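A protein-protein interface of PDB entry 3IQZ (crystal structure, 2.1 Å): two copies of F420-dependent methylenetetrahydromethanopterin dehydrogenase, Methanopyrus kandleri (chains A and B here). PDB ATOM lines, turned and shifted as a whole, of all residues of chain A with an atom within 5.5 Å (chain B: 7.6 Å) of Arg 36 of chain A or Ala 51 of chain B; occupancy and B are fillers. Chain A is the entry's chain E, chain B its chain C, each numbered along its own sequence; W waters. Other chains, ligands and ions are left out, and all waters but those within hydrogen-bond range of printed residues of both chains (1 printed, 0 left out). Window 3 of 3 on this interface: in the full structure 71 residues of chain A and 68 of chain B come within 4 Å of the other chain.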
ATOM      1  N   ALA A   6      15.750 -13.398   1.923  1.00  0.00           N
ATOM      2  CA  ALA A   6      14.721 -12.395   1.734  1.00  0.00           C
ATOM      3  C   ALA A   6      15.280 -10.990   1.982  1.00  0.00           C
ATOM      4  O   ALA A   6      16.221 -10.814   2.759  1.00  0.00           O
ATOM      5  CB  ALA A   6      13.552 -12.688   2.697  1.00  0.00           C
ATOM      6  N   ILE A   7      14.681  -9.982   1.374  1.00  0.00           N
ATOM      7  CA  ILE A   7      15.070  -8.623   1.685  1.00  0.00           C
ATOM      8  C   ILE A   7      13.839  -7.962   2.280  1.00  0.00           C
ATOM      9  O   ILE A   7      12.755  -8.072   1.679  1.00  0.00           O
ATOM     10  CB  ILE A   7      15.494  -7.823   0.421  1.00  0.00           C
ATOM     11  CG1 ILE A   7      16.702  -8.494  -0.274  1.00  0.00           C
ATOM     12  CG2 ILE A   7      15.807  -6.411   0.808  1.00  0.00           C
ATOM     13  CD1 ILE A   7      17.084  -7.898  -1.715  1.00  0.00           C
ATOM     14  N   PHE A   8      13.994  -7.299   3.429  1.00  0.00           N
ATOM     15  CA  PHE A   8      12.960  -6.460   4.007  1.00  0.00           C
ATOM     16  C   PHE A   8      13.176  -4.953   3.694  1.00  0.00           C
ATOM     17  O   PHE A   8      14.307  -4.441   3.772  1.00  0.00           O
ATOM     18  CB  PHE A   8      12.907  -6.698   5.523  1.00  0.00           C
ATOM     19  CG  PHE A   8      12.543  -8.108   5.896  1.00  0.00           C
ATOM     20  CD1 PHE A   8      13.485  -9.134   5.812  1.00  0.00           C
ATOM     21  CD2 PHE A   8      11.263  -8.415   6.322  1.00  0.00           C
ATOM     22  CE1 PHE A   8      13.165 -10.452   6.186  1.00  0.00           C
ATOM     23  CE2 PHE A   8      10.916  -9.730   6.722  1.00  0.00           C
ATOM     24  CZ  PHE A   8      11.860 -10.748   6.655  1.00  0.00           C
ATOM     25  N   GLU A  34      18.730 -16.077   5.510  1.00  0.00           N
ATOM     26  CA  GLU A  34      19.691 -14.987   5.476  1.00  0.00           C
ATOM     27  C   GLU A  34      18.968 -13.781   4.916  1.00  0.00           C
ATOM     28  O   GLU A  34      18.351 -13.869   3.847  1.00  0.00           O
ATOM     29  CB  GLU A  34      20.900 -15.341   4.604  1.00  0.00           C
ATOM     30  CG  GLU A  34      22.061 -14.373   4.775  1.00  0.00           C
ATOM     31  CD  GLU A  34      23.182 -14.611   3.779  1.00  0.00           C
ATOM     32  OE1 GLU A  34      24.159 -13.827   3.759  1.00  0.00           O
ATOM     33  OE2 GLU A  34      23.085 -15.574   2.994  1.00  0.00           O
ATOM     34  N   PHE A  35      19.065 -12.660   5.622  1.00  0.00           N
ATOM     35  CA  PHE A  35      18.236 -11.508   5.337  1.00  0.00           C
ATOM     36  C   PHE A  35      19.085 -10.282   5.063  1.00  0.00           C
ATOM     37  O   PHE A  35      20.194 -10.155   5.582  1.00  0.00           O
ATOM     38  CB  PHE A  35      17.277 -11.158   6.502  1.00  0.00           C
ATOM     39  CG  PHE A  35      16.353 -12.291   6.930  1.00  0.00           C
ATOM     40  CD1 PHE A  35      16.064 -12.495   8.296  1.00  0.00           C
ATOM     41  CD2 PHE A  35      15.733 -13.100   5.995  1.00  0.00           C
ATOM     42  CE1 PHE A  35      15.196 -13.559   8.698  1.00  0.00           C
ATOM     43  CE2 PHE A  35      14.898 -14.126   6.353  1.00  0.00           C
ATOM     44  CZ  PHE A  35      14.603 -14.365   7.696  1.00  0.00           C
ATOM     45  N   ARG A  36      18.529  -9.388   4.251  1.00  0.00           N
ATOM     46  CA  ARG A  36      19.016  -8.017   4.082  1.00  0.00           C
ATOM     47  C   ARG A  36      17.875  -7.061   4.466  1.00  0.00           C
ATOM     48  O   ARG A  36      16.702  -7.333   4.212  1.00  0.00           O
ATOM     49  CB  ARG A  36      19.456  -7.784   2.651  1.00  0.00           C
ATOM     50  CG  ARG A  36      20.662  -8.623   2.224  1.00  0.00           C
ATOM     51  CD  ARG A  36      21.904  -8.243   3.004  1.00  0.00           C
ATOM     52  NE  ARG A  36      23.042  -9.110   2.697  1.00  0.00           N
ATOM     53  CZ  ARG A  36      23.287 -10.255   3.330  1.00  0.00           C
ATOM     54  NH1 ARG A  36      24.342 -10.989   3.002  1.00  0.00           N
ATOM     55  NH2 ARG A  36      22.456 -10.682   4.278  1.00  0.00           N
ATOM     56  N   VAL A  37      18.203  -5.966   5.132  1.00  0.00           N
ATOM     57  CA  VAL A  37      17.191  -4.993   5.469  1.00  0.00           C
ATOM     58  C   VAL A  37      17.601  -3.631   4.942  1.00  0.00           C
ATOM     59  O   VAL A  37      18.748  -3.189   5.144  1.00  0.00           O
ATOM     60  CB  VAL A  37      16.994  -4.879   7.002  1.00  0.00           C
ATOM     61  CG1 VAL A  37      15.848  -3.956   7.323  1.00  0.00           C
ATOM     62  CG2 VAL A  37      16.753  -6.256   7.613  1.00  0.00           C
ATOM     63  N   VAL A  38      16.675  -2.955   4.280  1.00  0.00           N
ATOM     64  CA  VAL A  38      16.974  -1.640   3.777  1.00  0.00           C
ATOM     65  C   VAL A  38      15.761  -0.751   3.924  1.00  0.00           C
ATOM     66  O   VAL A  38      14.606  -1.209   3.953  1.00  0.00           O
ATOM     67  CB  VAL A  38      17.431  -1.641   2.261  1.00  0.00           C
ATOM     68  CG1 VAL A  38      18.634  -2.518   2.075  1.00  0.00           C
ATOM     69  CG2 VAL A  38      16.320  -2.077   1.314  1.00  0.00           C
ATOM     70  N   ILE A  59      20.592  -4.612  -4.611  1.00  0.00           N
ATOM     71  CA  ILE A  59      21.162  -5.671  -3.810  1.00  0.00           C
ATOM     72  C   ILE A  59      20.690  -7.031  -4.316  1.00  0.00           C
ATOM     73  O   ILE A  59      21.440  -8.003  -4.291  1.00  0.00           O
ATOM     74  CB  ILE A  59      20.790  -5.405  -2.333  1.00  0.00           C
ATOM     75  CG1 ILE A  59      21.699  -4.316  -1.768  1.00  0.00           C
ATOM     76  CG2 ILE A  59      20.769  -6.686  -1.461  1.00  0.00           C
ATOM     77  CD1 ILE A  59      21.039  -3.531  -0.653  1.00  0.00           C
ATOM     78  N   PHE A  63      22.254 -10.718  -4.405  1.00  0.00           N
ATOM     79  CA  PHE A  63      21.728 -11.476  -3.282  1.00  0.00           C
ATOM     80  C   PHE A  63      20.776 -12.578  -3.733  1.00  0.00           C
ATOM     81  O   PHE A  63      20.754 -13.652  -3.162  1.00  0.00           O
ATOM     82  CB  PHE A  63      21.017 -10.547  -2.282  1.00  0.00           C
ATOM     83  CG  PHE A  63      20.704 -11.194  -0.975  1.00  0.00           C
ATOM     84  CD1 PHE A  63      21.701 -11.795  -0.232  1.00  0.00           C
ATOM     85  CD2 PHE A  63      19.412 -11.170  -0.467  1.00  0.00           C
ATOM     86  CE1 PHE A  63      21.418 -12.379   0.991  1.00  0.00           C
ATOM     87  CE2 PHE A  63      19.112 -11.761   0.770  1.00  0.00           C
ATOM     88  CZ  PHE A  63      20.122 -12.368   1.489  1.00  0.00           C
ATOM     89  N   ILE B   9      23.589   1.490   9.999  1.00  0.00           N
ATOM     90  CA  ILE B   9      23.815   0.077   9.754  1.00  0.00           C
ATOM     91  C   ILE B   9      23.456  -0.659  11.043  1.00  0.00           C
ATOM     92  O   ILE B   9      23.992  -0.344  12.092  1.00  0.00           O
ATOM     93  CB  ILE B   9      25.301  -0.201   9.449  1.00  0.00           C
ATOM     94  CG1 ILE B   9      25.803   0.668   8.291  1.00  0.00           C
ATOM     95  CG2 ILE B   9      25.530  -1.710   9.166  1.00  0.00           C
ATOM     96  CD1 ILE B   9      27.306   0.699   8.103  1.00  0.00           C
ATOM     97  N   CYS B  11      23.229  -4.398  12.751  1.00  0.00           N
ATOM     98  CA  CYS B  11      23.485  -5.837  12.748  1.00  0.00           C
ATOM     99  C   CYS B  11      23.255  -6.315  14.197  1.00  0.00           C
ATOM    100  O   CYS B  11      23.837  -5.757  15.131  1.00  0.00           O
ATOM    101  CB  CYS B  11      24.905  -6.131  12.280  1.00  0.00           C
ATOM    102  SG  CYS B  11      25.191  -5.545  10.589  1.00  0.00           S
ATOM    103  N   VAL B  38      20.553   0.263   6.456  1.00  0.00           N
ATOM    104  CA  VAL B  38      20.806  -1.067   5.935  1.00  0.00           C
ATOM    105  C   VAL B  38      21.275  -1.958   7.054  1.00  0.00           C
ATOM    106  O   VAL B  38      21.737  -1.474   8.118  1.00  0.00           O
ATOM    107  CB  VAL B  38      21.880  -1.075   4.794  1.00  0.00           C
ATOM    108  CG1 VAL B  38      21.438  -0.228   3.625  1.00  0.00           C
ATOM    109  CG2 VAL B  38      23.192  -0.565   5.327  1.00  0.00           C
ATOM    110  N   GLY B  39      21.138  -3.261   6.833  1.00  0.00           N
ATOM    111  CA  GLY B  39      21.482  -4.228   7.880  1.00  0.00           C
ATOM    112  C   GLY B  39      21.299  -5.650   7.414  1.00  0.00           C
ATOM    113  O   GLY B  39      20.869  -5.895   6.277  1.00  0.00           O
ATOM    114  N   THR B  40      21.658  -6.590   8.295  1.00  0.00           N
ATOM    115  CA  THR B  40      21.563  -8.013   8.010  1.00  0.00           C
ATOM    116  C   THR B  40      20.707  -8.643   9.120  1.00  0.00           C
ATOM    117  O   THR B  40      20.941  -9.748   9.541  1.00  0.00           O
ATOM    118  CB  THR B  40      22.963  -8.689   7.953  1.00  0.00           C
ATOM    119  OG1 THR B  40      23.750  -8.282   9.078  1.00  0.00           O
ATOM    120  CG2 THR B  40      23.715  -8.296   6.662  1.00  0.00           C
ATOM    121  N   SER B  41      19.714  -7.895   9.578  1.00  0.00           N
ATOM    122  CA  SER B  41      18.804  -8.310  10.620  1.00  0.00           C
ATOM    123  C   SER B  41      19.590  -8.657  11.884  1.00  0.00           C
ATOM    124  O   SER B  41      20.569  -7.967  12.203  1.00  0.00           O
ATOM    125  CB  SER B  41      17.914  -9.469  10.152  1.00  0.00           C
ATOM    126  OG  SER B  41      16.881  -9.717  11.120  1.00  0.00           O
ATOM    127  N   LYS B  43      21.647 -11.052  12.488  1.00  0.00           N
ATOM    128  CA  LYS B  43      22.939 -11.751  12.370  1.00  0.00           C
ATOM    129  C   LYS B  43      24.107 -10.764  12.405  1.00  0.00           C
ATOM    130  O   LYS B  43      24.092  -9.773  11.677  1.00  0.00           O
ATOM    131  CB  LYS B  43      22.951 -12.615  11.099  1.00  0.00           C
ATOM    132  CG  LYS B  43      22.127 -13.929  11.293  1.00  0.00           C
ATOM    133  CD  LYS B  43      22.283 -14.866  10.075  1.00  0.00           C
ATOM    134  CE  LYS B  43      21.238 -15.976  10.094  1.00  0.00           C
ATOM    135  NZ  LYS B  43      21.101 -16.629  11.440  1.00  0.00           N
ATOM    136  N   ASP B  45      27.712 -11.938  13.025  1.00  0.00           N
ATOM    137  CA  ASP B  45      29.006 -12.568  12.799  1.00  0.00           C
ATOM    138  C   ASP B  45      29.799 -11.790  11.706  1.00  0.00           C
ATOM    139  O   ASP B  45      29.221 -10.995  10.940  1.00  0.00           O
ATOM    140  CB  ASP B  45      28.752 -13.995  12.321  1.00  0.00           C
ATOM    141  CG  ASP B  45      27.916 -14.022  11.024  1.00  0.00           C
ATOM    142  OD1 ASP B  45      26.707 -13.673  11.053  1.00  0.00           O
ATOM    143  OD2 ASP B  45      28.467 -14.359   9.968  1.00  0.00           O
ATOM    144  N   PRO B  46      31.123 -12.021  11.641  1.00  0.00           N
ATOM    145  CA  PRO B  46      32.001 -11.309  10.712  1.00  0.00           C
ATOM    146  C   PRO B  46      31.469 -11.200   9.279  1.00  0.00           C
ATOM    147  O   PRO B  46      31.477 -10.093   8.738  1.00  0.00           O
ATOM    148  CB  PRO B  46      33.297 -12.116  10.762  1.00  0.00           C
ATOM    149  CG  PRO B  46      33.327 -12.665  12.199  1.00  0.00           C
ATOM    150  CD  PRO B  46      31.876 -12.839  12.619  1.00  0.00           C
ATOM    151  N   GLU B  47      31.022 -12.295   8.654  1.00  0.00           N
ATOM    152  CA  GLU B  47      30.664 -12.213   7.207  1.00  0.00           C
ATOM    153  C   GLU B  47      29.459 -11.298   7.023  1.00  0.00           C
ATOM    154  O   GLU B  47      29.416 -10.491   6.090  1.00  0.00           O
ATOM    155  CB  GLU B  47      30.323 -13.577   6.580  1.00  0.00           C
ATOM    156  CG  GLU B  47      31.467 -14.575   6.455  1.00  0.00           C
ATOM    157  CD  GLU B  47      31.750 -15.303   7.771  1.00  0.00           C
ATOM    158  OE1 GLU B  47      31.138 -14.964   8.835  1.00  0.00           O
ATOM    159  OE2 GLU B  47      32.597 -16.221   7.748  1.00  0.00           O
ATOM    160  N   CYS B  48      28.465 -11.454   7.896  1.00  0.00           N
ATOM    161  CA  CYS B  48      27.268 -10.602   7.834  1.00  0.00           C
ATOM    162  C   CYS B  48      27.577  -9.144   8.068  1.00  0.00           C
ATOM    163  O   CYS B  48      27.098  -8.292   7.346  1.00  0.00           O
ATOM    164  CB  CYS B  48      26.256 -11.035   8.881  1.00  0.00           C
ATOM    165  SG  CYS B  48      25.786 -12.682   8.574  1.00  0.00           S
ATOM    166  N   VAL B  49      28.334  -8.857   9.122  1.00  0.00           N
ATOM    167  CA  VAL B  49      28.694  -7.482   9.396  1.00  0.00           C
ATOM    168  C   VAL B  49      29.435  -6.883   8.210  1.00  0.00           C
ATOM    169  O   VAL B  49      29.099  -5.787   7.788  1.00  0.00           O
ATOM    170  CB  VAL B  49      29.519  -7.322  10.681  1.00  0.00           C
ATOM    171  CG1 VAL B  49      29.962  -5.865  10.819  1.00  0.00           C
ATOM    172  CG2 VAL B  49      28.687  -7.759  11.874  1.00  0.00           C
ATOM    173  N   GLU B  50      30.431  -7.593   7.679  1.00  0.00           N
ATOM    174  CA  GLU B  50      31.156  -7.113   6.473  1.00  0.00           C
ATOM    175  C   GLU B  50      30.187  -6.833   5.319  1.00  0.00           C
ATOM    176  O   GLU B  50      30.289  -5.821   4.614  1.00  0.00           O
ATOM    177  CB  GLU B  50      32.272  -8.096   6.045  1.00  0.00           C
ATOM    178  CG  GLU B  50      32.973  -7.672   4.745  1.00  0.00           C
ATOM    179  CD  GLU B  50      34.122  -8.579   4.347  1.00  0.00           C
ATOM    180  OE1 GLU B  50      34.830  -8.251   3.383  1.00  0.00           O
ATOM    181  OE2 GLU B  50      34.317  -9.623   4.998  1.00  0.00           O
ATOM    182  N   ALA B  51      29.243  -7.739   5.116  1.00  0.00           N
ATOM    183  CA  ALA B  51      28.303  -7.592   4.017  1.00  0.00           C
ATOM    184  C   ALA B  51      27.433  -6.333   4.251  1.00  0.00           C
ATOM    185  O   ALA B  51      27.125  -5.569   3.317  1.00  0.00           O
ATOM    186  CB  ALA B  51      27.434  -8.837   3.941  1.00  0.00           C
ATOM    187  N   ALA B  52      27.028  -6.133   5.509  1.00  0.00           N
ATOM    188  CA  ALA B  52      26.249  -4.956   5.856  1.00  0.00           C
ATOM    189  C   ALA B  52      27.003  -3.656   5.594  1.00  0.00           C
ATOM    190  O   ALA B  52      26.447  -2.712   5.035  1.00  0.00           O
ATOM    191  CB  ALA B  52      25.714  -5.037   7.383  1.00  0.00           C
ATOM    192  N   VAL B  53      28.277  -3.605   5.959  1.00  0.00           N
ATOM    193  CA  VAL B  53      29.064  -2.391   5.789  1.00  0.00           C
ATOM    194  C   VAL B  53      29.353  -2.119   4.290  1.00  0.00           C
ATOM    195  O   VAL B  53      29.440  -0.962   3.845  1.00  0.00           O
ATOM    196  CB  VAL B  53      30.375  -2.457   6.609  1.00  0.00           C
ATOM    197  CG1 VAL B  53      31.167  -1.190   6.430  1.00  0.00           C
ATOM    198  CG2 VAL B  53      30.109  -2.716   8.103  1.00  0.00           C
ATOM    199  N   GLU B  54      29.486  -3.187   3.506  1.00  0.00           N
ATOM    200  CA  GLU B  54      29.638  -3.046   2.064  1.00  0.00           C
ATOM    201  C   GLU B  54      28.412  -2.434   1.398  1.00  0.00           C
ATOM    202  O   GLU B  54      28.529  -1.593   0.506  1.00  0.00           O
ATOM    203  CB  GLU B  54      29.949  -4.397   1.443  1.00  0.00           C
ATOM    204  CG  GLU B  54      31.382  -4.773   1.666  1.00  0.00           C
ATOM    205  CD  GLU B  54      31.853  -5.884   0.771  1.00  0.00           C
ATOM    206  OE1 GLU B  54      31.633  -5.796  -0.459  1.00  0.00           O
ATOM    207  OE2 GLU B  54      32.464  -6.847   1.309  1.00  0.00           O
ATOM    208  N   MET B  55      27.226  -2.849   1.844  1.00  0.00           N
ATOM    209  CA  MET B  55      25.994  -2.257   1.323  1.00  0.00           C
ATOM    210  C   MET B  55      26.044  -0.774   1.596  1.00  0.00           C
ATOM    211  O   MET B  55      25.873   0.055   0.689  1.00  0.00           O
ATOM    212  CB  MET B  55      24.778  -2.812   2.014  1.00  0.00           C
ATOM    213  CG  MET B  55      24.351  -4.171   1.546  1.00  0.00           C
ATOM    214  SD  MET B  55      22.711  -4.503   2.223  1.00  0.00           S
ATOM    215  CE  MET B  55      23.040  -4.689   3.973  1.00  0.00           C
ATOM    216  N   ALA B  56      26.327  -0.453   2.847  1.00  0.00           N
ATOM    217  CA  ALA B  56      26.453   0.931   3.249  1.00  0.00           C
ATOM    218  C   ALA B  56      27.431   1.674   2.328  1.00  0.00           C
ATOM    219  O   ALA B  56      27.088   2.718   1.821  1.00  0.00           O
ATOM    220  CB  ALA B  56      26.881   1.052   4.690  1.00  0.00           C
ATOM    221  N   LEU B  57      28.650   1.167   2.204  1.00  0.00           N
ATOM    222  CA  LEU B  57      29.677   1.838   1.380  1.00  0.00           C
ATOM    223  C   LEU B  57      29.320   1.897  -0.106  1.00  0.00           C
ATOM    224  O   LEU B  57      29.638   2.857  -0.791  1.00  0.00           O
ATOM    225  CB  LEU B  57      31.060   1.202   1.596  1.00  0.00           C
ATOM    226  CG  LEU B  57      31.469   1.289   3.086  1.00  0.00           C
ATOM    227  CD1 LEU B  57      32.728   0.485   3.365  1.00  0.00           C
ATOM    228  CD2 LEU B  57      31.636   2.752   3.545  1.00  0.00           C
ATOM    229  N   ASP B  58      28.678   0.862  -0.623  1.00  0.00           N
ATOM    230  CA  ASP B  58      28.242   0.918  -2.020  1.00  0.00           C
ATOM    231  C   ASP B  58      27.252   2.063  -2.196  1.00  0.00           C
ATOM    232  O   ASP B  58      27.382   2.881  -3.112  1.00  0.00           O
ATOM    233  CB  ASP B  58      27.591  -0.396  -2.445  1.00  0.00           C
ATOM    234  CG  ASP B  58      28.592  -1.535  -2.544  1.00  0.00           C
ATOM    235  OD1 ASP B  58      29.800  -1.264  -2.629  1.00  0.00           O
ATOM    236  OD2 ASP B  58      28.179  -2.709  -2.543  1.00  0.00           O
ATOM    237  N   LYS B  82      35.063  -5.965  13.017  1.00  0.00           N
ATOM    238  CA  LYS B  82      35.248  -5.836  11.597  1.00  0.00           C
ATOM    239  C   LYS B  82      34.620  -4.529  11.116  1.00  0.00           C
ATOM    240  O   LYS B  82      35.202  -3.802  10.353  1.00  0.00           O
ATOM    241  CB  LYS B  82      34.628  -7.046  10.884  1.00  0.00           C
ATOM    242  CG  LYS B  82      34.961  -7.120   9.408  1.00  0.00           C
ATOM    243  CD  LYS B  82      36.268  -7.853   9.180  1.00  0.00           C
ATOM    244  CE  LYS B  82      36.326  -8.397   7.774  1.00  0.00           C
ATOM    245  NZ  LYS B  82      37.353  -7.712   6.968  1.00  0.00           N
ATOM    246  N   MET B  86      36.541  -1.417   9.197  1.00  0.00           N
ATOM    247  CA  MET B  86      36.137  -0.922   7.878  1.00  0.00           C
ATOM    248  C   MET B  86      35.730   0.539   7.969  1.00  0.00           C
ATOM    249  O   MET B  86      36.093   1.343   7.130  1.00  0.00           O
ATOM    250  CB  MET B  86      34.986  -1.754   7.318  1.00  0.00           C
ATOM    251  CG  MET B  86      35.328  -3.220   7.169  1.00  0.00           C
ATOM    252  SD  MET B  86      33.952  -4.312   6.736  1.00  0.00           S
ATOM    253  CE  MET B  86      33.617  -3.774   5.038  1.00  0.00           C
HETATM  254  O   HOH W   1      23.663 -12.981   6.798  1.00  0.00           O
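The backbone carbonyl oxygen (O) of Gly 39 of chain B is in hydrogen-bond range of the backbone NH (N) of Val 37 of chain A.
The guanidinium group of Arg 36 of chain A is in salt-bridge range of the side-chain carboxylate of Glu 34 of chain A, 2.9 Å away.
N of Phe 8 of chain A lies within hydrogen-bond range of O of Arg 36 of chain A (2.8 Å).
N of Val 38 of chain A lies within hydrogen-bond range of O of Phe 8 of chain A, 2.8 Å away.
The side-chain sulfur (SG) of Cys 11 of chain B sits at hydrogen-bond distance from the side-chain hydroxyl (OG1) of Thr 40 of chain B.
N of Arg 36 of chain A sits at hydrogen-bond distance from O of Ala 6 of chain A, at 3.1 Å.
The side-chain hydroxyl (OG1) of Thr 40 of chain B is in hydrogen-bond range of the backbone carbonyl oxygen (O) of Lys 43 of chain B (3.0 Å).
Phe 35 of chain A touches Thr 40 of chain B.
O of Gly 39 of chain B touches CA of Arg 36 of chain A (3.6 Å).
Arg 36 of chain A touches Thr 40 of chain B (NH2 to CG2, 3.6 Å).
Arg 36 of chain A touches Ala 51 of chain B.
CD of Arg 36 of chain A touches CE of Met 55 of chain B (3.9 Å).
Val 37 of chain A touches Val 38 of chain B (O to CA, 3.1 Å).
CG2 of Val 37 of chain A touches N of Ser 41 of chain B, 3.9 Å away.
CG1 of Val 38 of chain A touches CG1 of Val 38 of chain B, 3.9 Å away.
SD of Met 55 of chain B touches CD1 of Ile 59 of chain A (3.5 Å).
Of the printed residues of chain B, Ile 59 of chain A touches Met 55 (3.5 Å).
Printed residues of chain A within 4 Å of Gly 39 of chain B: Arg 36 and Val 37.
Of the printed residues of chain A, Ala 51 of chain B touches Arg 36 (3.9 Å).
The nearest printed residue of chain A that does not touch Ala 51 of chain B is Glu 34 of chain A (6.0 Å).
Of the 10 printed residues of chain A, 5 touch a printed residue of chain B.
Hydrophobic or aromatic side chains of chain A within 4 Å of the printed part of chain B: Val 37, Val 38 and Ile 59.
Along chain A the printed residues that touch a printed residue of chain B span positions 35 to 59.
Printed residues of chain B that touch a printed residue of chain A: Val 38, Gly 39, Thr 40, Ser 41, Ala 51 and Met 55.
Hydrophobic or aromatic side chains of chain B within 4 Å of the printed part of chain A: Val 38, Ala 51 and Met 55.
Among the printed residues, no Asp or Glu carboxylate lies within 4 Å of a Lys or Arg side-chain nitrogen of the other chain.
Val 38 of chain B touches its own counterpart, Val 38 of chain A.
Position printed for both chains: 38.
Of the 10 pairs that touch across the chains among the printed residues, 1 has its exchanged pair printed and touching as well.
Water W1 bridges the side-chain sulfur of Cys 48 of chain B (2.8 Å) and the side-chain carboxylate of Glu 34 of chain A (3.2 Å).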
